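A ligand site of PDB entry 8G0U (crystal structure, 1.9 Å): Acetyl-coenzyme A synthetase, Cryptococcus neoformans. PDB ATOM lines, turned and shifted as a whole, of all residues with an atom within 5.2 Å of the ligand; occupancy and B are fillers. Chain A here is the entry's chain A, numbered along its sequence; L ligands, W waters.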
ATOM      1  N   THR A 303      15.678   5.782  31.137  1.00  0.00           N
ATOM      2  CA  THR A 303      14.590   6.611  30.654  1.00  0.00           C
ATOM      3  C   THR A 303      14.445   7.847  31.536  1.00  0.00           C
ATOM      4  O   THR A 303      14.916   7.886  32.680  1.00  0.00           O
ATOM      5  CB  THR A 303      13.273   5.834  30.664  1.00  0.00           C
ATOM      6  OG1 THR A 303      12.940   5.507  32.014  1.00  0.00           O
ATOM      7  CG2 THR A 303      13.359   4.576  29.833  1.00  0.00           C
ATOM      8  N   TRP A 348      17.475   6.025  22.192  1.00  0.00           N
ATOM      9  CA  TRP A 348      16.104   5.609  22.482  1.00  0.00           C
ATOM     10  C   TRP A 348      15.980   4.107  22.280  1.00  0.00           C
ATOM     11  O   TRP A 348      16.680   3.537  21.441  1.00  0.00           O
ATOM     12  CB  TRP A 348      15.151   6.345  21.535  1.00  0.00           C
ATOM     13  CG  TRP A 348      13.688   6.362  21.884  1.00  0.00           C
ATOM     14  CD1 TRP A 348      13.109   6.094  23.097  1.00  0.00           C
ATOM     15  CD2 TRP A 348      12.619   6.668  20.987  1.00  0.00           C
ATOM     16  NE1 TRP A 348      11.734   6.226  22.999  1.00  0.00           N
ATOM     17  CE2 TRP A 348      11.414   6.583  21.717  1.00  0.00           C
ATOM     18  CE3 TRP A 348      12.569   7.017  19.634  1.00  0.00           C
ATOM     19  CZ2 TRP A 348      10.172   6.834  21.126  1.00  0.00           C
ATOM     20  CZ3 TRP A 348      11.334   7.270  19.049  1.00  0.00           C
ATOM     21  CH2 TRP A 348      10.147   7.176  19.805  1.00  0.00           C
ATOM     22  N   ILE A 349      15.089   3.474  23.038  1.00  0.00           N
ATOM     23  CA  ILE A 349      14.890   2.045  22.868  1.00  0.00           C
ATOM     24  C   ILE A 349      14.539   1.743  21.412  1.00  0.00           C
ATOM     25  O   ILE A 349      14.893   0.675  20.888  1.00  0.00           O
ATOM     26  CB  ILE A 349      13.800   1.511  23.822  1.00  0.00           C
ATOM     27  CG1 ILE A 349      13.742  -0.020  23.790  1.00  0.00           C
ATOM     28  CG2 ILE A 349      12.432   2.073  23.451  1.00  0.00           C
ATOM     29  CD1 ILE A 349      14.946  -0.737  24.492  1.00  0.00           C
ATOM     30  N   THR A 350      13.848   2.663  20.735  1.00  0.00           N
ATOM     31  CA  THR A 350      13.532   2.444  19.326  1.00  0.00           C
ATOM     32  C   THR A 350      14.787   2.218  18.496  1.00  0.00           C
ATOM     33  O   THR A 350      14.798   1.408  17.574  1.00  0.00           O
ATOM     34  CB  THR A 350      12.740   3.636  18.782  1.00  0.00           C
ATOM     35  OG1 THR A 350      11.572   3.836  19.586  1.00  0.00           O
ATOM     36  CG2 THR A 350      12.335   3.372  17.358  1.00  0.00           C
ATOM     37  N   SER A 424       4.902   4.002  12.805  1.00  0.00           N
ATOM     38  CA  SER A 424       4.803   5.141  13.717  1.00  0.00           C
ATOM     39  C   SER A 424       4.947   4.638  15.153  1.00  0.00           C
ATOM     40  O   SER A 424       4.282   3.667  15.534  1.00  0.00           O
ATOM     41  CB  SER A 424       3.449   5.859  13.530  1.00  0.00           C
ATOM     42  OG  SER A 424       3.265   6.889  14.481  1.00  0.00           O
ATOM     43  N   VAL A 425       5.797   5.298  15.935  1.00  0.00           N
ATOM     44  CA  VAL A 425       6.064   4.867  17.316  1.00  0.00           C
ATOM     45  C   VAL A 425       6.297   6.092  18.190  1.00  0.00           C
ATOM     46  O   VAL A 425       6.911   7.072  17.771  1.00  0.00           O
ATOM     47  CB  VAL A 425       7.281   3.922  17.375  1.00  0.00           C
ATOM     48  CG1 VAL A 425       8.522   4.597  16.785  1.00  0.00           C
ATOM     49  CG2 VAL A 425       7.547   3.512  18.810  1.00  0.00           C
ATOM     50  N   GLY A 426       5.821   6.022  19.443  1.00  0.00           N
ATOM     51  CA  GLY A 426       6.225   6.996  20.441  1.00  0.00           C
ATOM     52  C   GLY A 426       5.071   7.592  21.218  1.00  0.00           C
ATOM     53  O   GLY A 426       5.199   7.933  22.402  1.00  0.00           O
ATOM     54  N   GLU A 427       3.933   7.735  20.557  1.00  0.00           N
ATOM     55  CA  GLU A 427       2.737   8.302  21.167  1.00  0.00           C
ATOM     56  C   GLU A 427       1.548   7.967  20.271  1.00  0.00           C
ATOM     57  O   GLU A 427       1.729   7.485  19.148  1.00  0.00           O
ATOM     58  CB  GLU A 427       2.865   9.830  21.359  1.00  0.00           C
ATOM     59  CG  GLU A 427       3.314  10.247  22.763  1.00  0.00           C
ATOM     60  CD  GLU A 427       3.027  11.711  23.090  1.00  0.00           C
ATOM     61  OE1 GLU A 427       2.378  12.413  22.272  1.00  0.00           O
ATOM     62  OE2 GLU A 427       3.453  12.161  24.177  1.00  0.00           O
ATOM     63  N   PRO A 428       0.332   8.203  20.740  1.00  0.00           N
ATOM     64  CA  PRO A 428      -0.821   8.079  19.848  1.00  0.00           C
ATOM     65  C   PRO A 428      -0.618   8.934  18.619  1.00  0.00           C
ATOM     66  O   PRO A 428      -0.132  10.068  18.703  1.00  0.00           O
ATOM     67  CB  PRO A 428      -2.004   8.561  20.694  1.00  0.00           C
ATOM     68  CG  PRO A 428      -1.556   8.362  22.101  1.00  0.00           C
ATOM     69  CD  PRO A 428      -0.070   8.613  22.105  1.00  0.00           C
ATOM     70  N   ASP A 450       1.085   1.229  13.180  1.00  0.00           N
ATOM     71  CA  ASP A 450       1.126   1.971  14.439  1.00  0.00           C
ATOM     72  C   ASP A 450       1.588   1.018  15.530  1.00  0.00           C
ATOM     73  O   ASP A 450       0.841   0.119  15.937  1.00  0.00           O
ATOM     74  CB  ASP A 450      -0.267   2.566  14.680  1.00  0.00           C
ATOM     75  CG  ASP A 450      -0.361   3.380  15.961  1.00  0.00           C
ATOM     76  OD1 ASP A 450       0.660   3.581  16.638  1.00  0.00           O
ATOM     77  OD2 ASP A 450      -1.478   3.843  16.267  1.00  0.00           O
ATOM     78  N   THR A 451       2.838   1.160  15.986  1.00  0.00           N
ATOM     79  CA  THR A 451       3.462   0.182  16.874  1.00  0.00           C
ATOM     80  C   THR A 451       3.486   0.707  18.299  1.00  0.00           C
ATOM     81  O   THR A 451       4.160   1.700  18.597  1.00  0.00           O
ATOM     82  CB  THR A 451       4.890  -0.126  16.421  1.00  0.00           C
ATOM     83  OG1 THR A 451       5.696   1.048  16.574  1.00  0.00           O
ATOM     84  CG2 THR A 451       4.916  -0.549  14.966  1.00  0.00           C
ATOM     85  N   TYR A 452       2.759   0.027  19.187  1.00  0.00           N
ATOM     86  CA  TYR A 452       2.748   0.377  20.599  1.00  0.00           C
ATOM     87  C   TYR A 452       3.685  -0.530  21.382  1.00  0.00           C
ATOM     88  O   TYR A 452       3.625  -1.755  21.244  1.00  0.00           O
ATOM     89  CB  TYR A 452       1.340   0.281  21.191  1.00  0.00           C
ATOM     90  CG  TYR A 452       1.358   0.351  22.691  1.00  0.00           C
ATOM     91  CD1 TYR A 452       1.496   1.560  23.345  1.00  0.00           C
ATOM     92  CD2 TYR A 452       1.268  -0.806  23.465  1.00  0.00           C
ATOM     93  CE1 TYR A 452       1.531   1.627  24.728  1.00  0.00           C
ATOM     94  CE2 TYR A 452       1.288  -0.742  24.833  1.00  0.00           C
ATOM     95  CZ  TYR A 452       1.424   0.472  25.460  1.00  0.00           C
ATOM     96  OH  TYR A 452       1.444   0.536  26.829  1.00  0.00           O
ATOM     97  N   TRP A 453       4.538   0.069  22.204  1.00  0.00           N
ATOM     98  CA  TRP A 453       5.412  -0.660  23.116  1.00  0.00           C
ATOM     99  C   TRP A 453       6.091   0.367  24.023  1.00  0.00           C
ATOM    100  O   TRP A 453       5.750   1.564  23.985  1.00  0.00           O
ATOM    101  CB  TRP A 453       6.419  -1.535  22.346  1.00  0.00           C
ATOM    102  CG  TRP A 453       7.283  -0.819  21.338  1.00  0.00           C
ATOM    103  CD1 TRP A 453       6.877  -0.118  20.244  1.00  0.00           C
ATOM    104  CD2 TRP A 453       8.718  -0.783  21.324  1.00  0.00           C
ATOM    105  NE1 TRP A 453       7.968   0.362  19.560  1.00  0.00           N
ATOM    106  CE2 TRP A 453       9.107  -0.028  20.200  1.00  0.00           C
ATOM    107  CE3 TRP A 453       9.710  -1.316  22.159  1.00  0.00           C
ATOM    108  CZ2 TRP A 453      10.449   0.215  19.890  1.00  0.00           C
ATOM    109  CZ3 TRP A 453      11.052  -1.073  21.849  1.00  0.00           C
ATOM    110  CH2 TRP A 453      11.401  -0.312  20.722  1.00  0.00           C
ATOM    111  N   MET A 454       7.051  -0.106  24.821  1.00  0.00           N
ATOM    112  CA  MET A 454       7.773   0.722  25.770  1.00  0.00           C
ATOM    113  C   MET A 454       9.198   0.205  25.914  1.00  0.00           C
ATOM    114  O   MET A 454       9.501  -0.940  25.561  1.00  0.00           O
ATOM    115  CB  MET A 454       7.106   0.711  27.163  1.00  0.00           C
ATOM    116  CG  MET A 454       5.605   0.949  27.157  1.00  0.00           C
ATOM    117  SD  MET A 454       4.981   1.231  28.819  1.00  0.00           S
ATOM    118  CE  MET A 454       5.597  -0.215  29.671  1.00  0.00           C
ATOM    119  N   THR A 455      10.071   1.069  26.441  1.00  0.00           N
ATOM    120  CA  THR A 455      11.423   0.639  26.771  1.00  0.00           C
ATOM    121  C   THR A 455      11.375  -0.660  27.576  1.00  0.00           C
ATOM    122  O   THR A 455      12.132  -1.606  27.309  1.00  0.00           O
ATOM    123  CB  THR A 455      12.148   1.739  27.572  1.00  0.00           C
ATOM    124  OG1 THR A 455      12.217   2.951  26.809  1.00  0.00           O
ATOM    125  CG2 THR A 455      13.562   1.291  27.959  1.00  0.00           C
ATOM    126  N   GLU A 456      10.420  -0.739  28.511  1.00  0.00           N
ATOM    127  CA  GLU A 456      10.320  -1.889  29.395  1.00  0.00           C
ATOM    128  C   GLU A 456       9.794  -3.140  28.711  1.00  0.00           C
ATOM    129  O   GLU A 456       9.888  -4.228  29.297  1.00  0.00           O
ATOM    130  CB  GLU A 456       9.406  -1.540  30.572  1.00  0.00           C
ATOM    131  CG  GLU A 456       9.923  -0.432  31.455  1.00  0.00           C
ATOM    132  CD  GLU A 456       9.437   0.947  31.035  1.00  0.00           C
ATOM    133  OE1 GLU A 456       9.118   1.133  29.846  1.00  0.00           O
ATOM    134  OE2 GLU A 456       9.378   1.837  31.902  1.00  0.00           O
ATOM    135  N   PHE A 539       1.251  -1.358  32.131  1.00  0.00           N
ATOM    136  CA  PHE A 539       1.962  -0.527  31.169  1.00  0.00           C
ATOM    137  C   PHE A 539       1.989   0.952  31.562  1.00  0.00           C
ATOM    138  O   PHE A 539       2.937   1.657  31.222  1.00  0.00           O
ATOM    139  CB  PHE A 539       1.327  -0.638  29.774  1.00  0.00           C
ATOM    140  CG  PHE A 539       1.511  -1.965  29.104  1.00  0.00           C
ATOM    141  CD1 PHE A 539       0.639  -3.007  29.366  1.00  0.00           C
ATOM    142  CD2 PHE A 539       2.531  -2.159  28.189  1.00  0.00           C
ATOM    143  CE1 PHE A 539       0.776  -4.219  28.733  1.00  0.00           C
ATOM    144  CE2 PHE A 539       2.692  -3.373  27.562  1.00  0.00           C
ATOM    145  CZ  PHE A 539       1.810  -4.410  27.833  1.00  0.00           C
ATOM    146  N   ASP A 541      -0.597   3.037  30.548  1.00  0.00           N
ATOM    147  CA  ASP A 541      -1.362   3.703  29.509  1.00  0.00           C
ATOM    148  C   ASP A 541      -2.834   3.328  29.606  1.00  0.00           C
ATOM    149  O   ASP A 541      -3.167   2.179  29.904  1.00  0.00           O
ATOM    150  CB  ASP A 541      -0.850   3.308  28.131  1.00  0.00           C
ATOM    151  CG  ASP A 541       0.532   3.810  27.869  1.00  0.00           C
ATOM    152  OD1 ASP A 541       0.717   5.044  27.834  1.00  0.00           O
ATOM    153  OD2 ASP A 541       1.447   2.965  27.694  1.00  0.00           O
ATOM    154  N   ILE A 553      -4.695   2.749  22.088  1.00  0.00           N
ATOM    155  CA  ILE A 553      -3.883   3.264  23.187  1.00  0.00           C
ATOM    156  C   ILE A 553      -3.953   4.788  23.105  1.00  0.00           C
ATOM    157  O   ILE A 553      -3.406   5.382  22.173  1.00  0.00           O
ATOM    158  CB  ILE A 553      -2.423   2.787  23.098  1.00  0.00           C
ATOM    159  CG1 ILE A 553      -2.344   1.293  22.774  1.00  0.00           C
ATOM    160  CG2 ILE A 553      -1.729   3.107  24.387  1.00  0.00           C
ATOM    161  CD1 ILE A 553      -3.075   0.400  23.727  1.00  0.00           C
ATOM    162  N   GLY A 555      -3.241   7.392  25.522  1.00  0.00           N
ATOM    163  CA  GLY A 555      -2.475   8.279  26.370  1.00  0.00           C
ATOM    164  C   GLY A 555      -2.131   7.639  27.688  1.00  0.00           C
ATOM    165  O   GLY A 555      -2.627   6.573  28.063  1.00  0.00           O
ATOM    166  N   ARG A 556      -1.255   8.330  28.423  1.00  0.00           N
ATOM    167  CA  ARG A 556      -0.827   7.857  29.735  1.00  0.00           C
ATOM    168  C   ARG A 556      -1.989   7.914  30.723  1.00  0.00           C
ATOM    169  O   ARG A 556      -2.859   8.795  30.643  1.00  0.00           O
ATOM    170  CB  ARG A 556       0.345   8.701  30.251  1.00  0.00           C
ATOM    171  CG  ARG A 556       1.640   8.600  29.426  1.00  0.00           C
ATOM    172  CD  ARG A 556       2.301   7.239  29.563  1.00  0.00           C
ATOM    173  NE  ARG A 556       2.733   6.945  30.919  1.00  0.00           N
ATOM    174  CZ  ARG A 556       3.169   5.766  31.334  1.00  0.00           C
ATOM    175  NH1 ARG A 556       3.254   4.736  30.513  1.00  0.00           N
ATOM    176  NH2 ARG A 556       3.554   5.625  32.604  1.00  0.00           N
ATOM    177  N   SER A 652      13.084  12.417  22.100  1.00  0.00           N
ATOM    178  CA  SER A 652      12.445  11.404  21.264  1.00  0.00           C
ATOM    179  C   SER A 652      11.090  11.838  20.734  1.00  0.00           C
ATOM    180  O   SER A 652      10.535  11.164  19.855  1.00  0.00           O
ATOM    181  CB  SER A 652      12.296  10.090  22.045  1.00  0.00           C
ATOM    182  OG  SER A 652      11.400  10.245  23.130  1.00  0.00           O
HETATM  183  C1  LIG L   1       4.154   4.265  26.180  1.00  0.00           C
HETATM  184  C2  LIG L   1       3.053   5.201  25.688  1.00  0.00           C
HETATM  185  C3  LIG L   1       3.747   5.881  24.514  1.00  0.00           C
HETATM  186  C4  LIG L   1       4.554   4.637  22.438  1.00  0.00           C
HETATM  187  C5  LIG L   1       2.735   4.421  21.365  1.00  0.00           C
HETATM  188  C6  LIG L   1       2.403   5.085  22.531  1.00  0.00           C
HETATM  189  O1  LIG L   1       4.026   3.865  27.539  1.00  0.00           O
HETATM  190  C7  LIG L   1       0.276   5.202  21.975  1.00  0.00           C
HETATM  191  C8  LIG L   1       1.681   4.165  20.458  1.00  0.00           C
HETATM  192  C9  LIG L   1       5.392   5.140  26.013  1.00  0.00           C
HETATM  193  C10 LIG L   1       6.699   4.384  25.910  1.00  0.00           C
HETATM  194  C11 LIG L   1       9.234   3.872  23.124  1.00  0.00           C
HETATM  195  C12 LIG L   1       9.003   2.589  22.378  1.00  0.00           C
HETATM  196  C13 LIG L   1       8.204   4.899  22.814  1.00  0.00           C
HETATM  197  O2  LIG L   1       5.143   5.906  24.803  1.00  0.00           O
HETATM  198  O3  LIG L   1       2.711   6.187  26.650  1.00  0.00           O
HETATM  199  O4  LIG L   1       7.798   5.303  25.790  1.00  0.00           O
HETATM  200  O5  LIG L   1       9.564   3.940  26.966  1.00  0.00           O
HETATM  201  N1  LIG L   1       3.582   5.217  23.220  1.00  0.00           N
HETATM  202  O6  LIG L   1       9.169   3.582  24.554  1.00  0.00           O
HETATM  203  N2  LIG L   1       0.443   4.569  20.813  1.00  0.00           N
HETATM  204  O7  LIG L   1      10.138   5.811  25.299  1.00  0.00           O
HETATM  205  N3  LIG L   1       4.090   4.147  21.311  1.00  0.00           N
HETATM  206  N4  LIG L   1       1.188   5.507  22.901  1.00  0.00           N
HETATM  207  N5  LIG L   1       1.854   3.536  19.289  1.00  0.00           N
HETATM  208  P1  LIG L   1       9.263   4.683  25.712  1.00  0.00           P
HETATM  209  O   HOH W   1      -1.069   3.160  19.306  1.00  0.00           O
HETATM  210  O   HOH W   2       1.596   8.537  25.147  1.00  0.00           O
HETATM  211  O   HOH W   3       9.255   8.328  25.633  1.00  0.00           O
HETATM  212  O   HOH W   4      -0.167   6.248  25.343  1.00  0.00           O
HETATM  213  O   HOH W   5       8.659   3.851  29.312  1.00  0.00           O
HETATM  214  O   HOH W   6      12.052   6.672  27.452  1.00  0.00           O
HETATM  215  O   HOH W   7       5.934   4.852  29.541  1.00  0.00           O
HETATM  216  O   HOH W   8       4.456   8.571  27.319  1.00  0.00           O
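N of Gly 426 sits at hydrogen-bond distance from N3 of the ligand, at 3.2 Å. O1 of the ligand lies within hydrogen-bond range of SD of Met 454. The backbone carbonyl oxygen of Thr 451 sits at hydrogen-bond distance from a nitrogen (N5) of the ligand (3.0 Å). An oxygen (O7) of the ligand is in hydrogen-bond range of the indole nitrogen (NE1) of Trp 348 (2.8 Å). An oxygen (O3) of the ligand is in hydrogen-bond range of the side-chain carboxylate (OD1) of Asp 541, at 2.6 Å. The side-chain carboxylate (OD1) of Asp 450 sits at hydrogen-bond distance from a nitrogen (N5) of the ligand, 2.9 Å away. N of Thr 455 lies within hydrogen-bond range of O5 of the ligand, 3.0 Å away. NH1 of Arg 556 is in hydrogen-bond range of O1 of the ligand (3.2 Å). The side-chain hydroxyl of Thr 455 is in hydrogen-bond range of an oxygen (O5) of the ligand, at 2.8 Å.
The backbone NH (N) of Thr 451 lies within hydrogen-bond range of the backbone carbonyl oxygen (O) of Ser 424. The guanidinium group (NH1) of Arg 556 lies within salt-bridge range of the side-chain carboxylate (OD1) of Asp 541 (3.7 Å). The side-chain hydroxyl of Tyr 452 sits at hydrogen-bond distance from the side-chain carboxylate of Asp 541 (2.6 Å). The guanidinium group of Arg 556 sits at hydrogen-bond distance from the backbone carbonyl oxygen of Phe 539 (3.2 Å).
Ile 349 touches the ligand (CG2 to C12, 3.6 Å). OG1 of Thr 350 touches C12 of the ligand, at 3.99 Å. Val 425 touches the ligand. C of Glu 427 touches C7 of the ligand, at 3.5 Å. Pro 428 touches the ligand (N to C7, 3.2 Å). CA of Tyr 452 touches N5 of the ligand, 3.5 Å away. Trp 453 touches the ligand. Ile 553 touches the ligand (O to C7, 3.7 Å). Along chain A the residues within 4 Å of the ligand span positions 348 to 556. The nearest printed residue that does not touch the ligand is Glu 456 (4.05 Å).
Water W5 lies within hydrogen-bond range of an oxygen (O5) of the ligand and the side-chain carboxylate of Glu 456. Water W1 lies within hydrogen-bond range of N2 of the ligand (2.6 Å) and OD2 of Asp 450 (3.1 Å). Water W4 lies within hydrogen-bond range of N4 of the ligand (2.9 Å), OD1 of Asp 541 (2.9 Å) and N of Gly 555 (3.3 Å). Water W7 bridges NH1 of Arg 556 (2.9 Å) and O1 of the ligand (2.9 Å).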
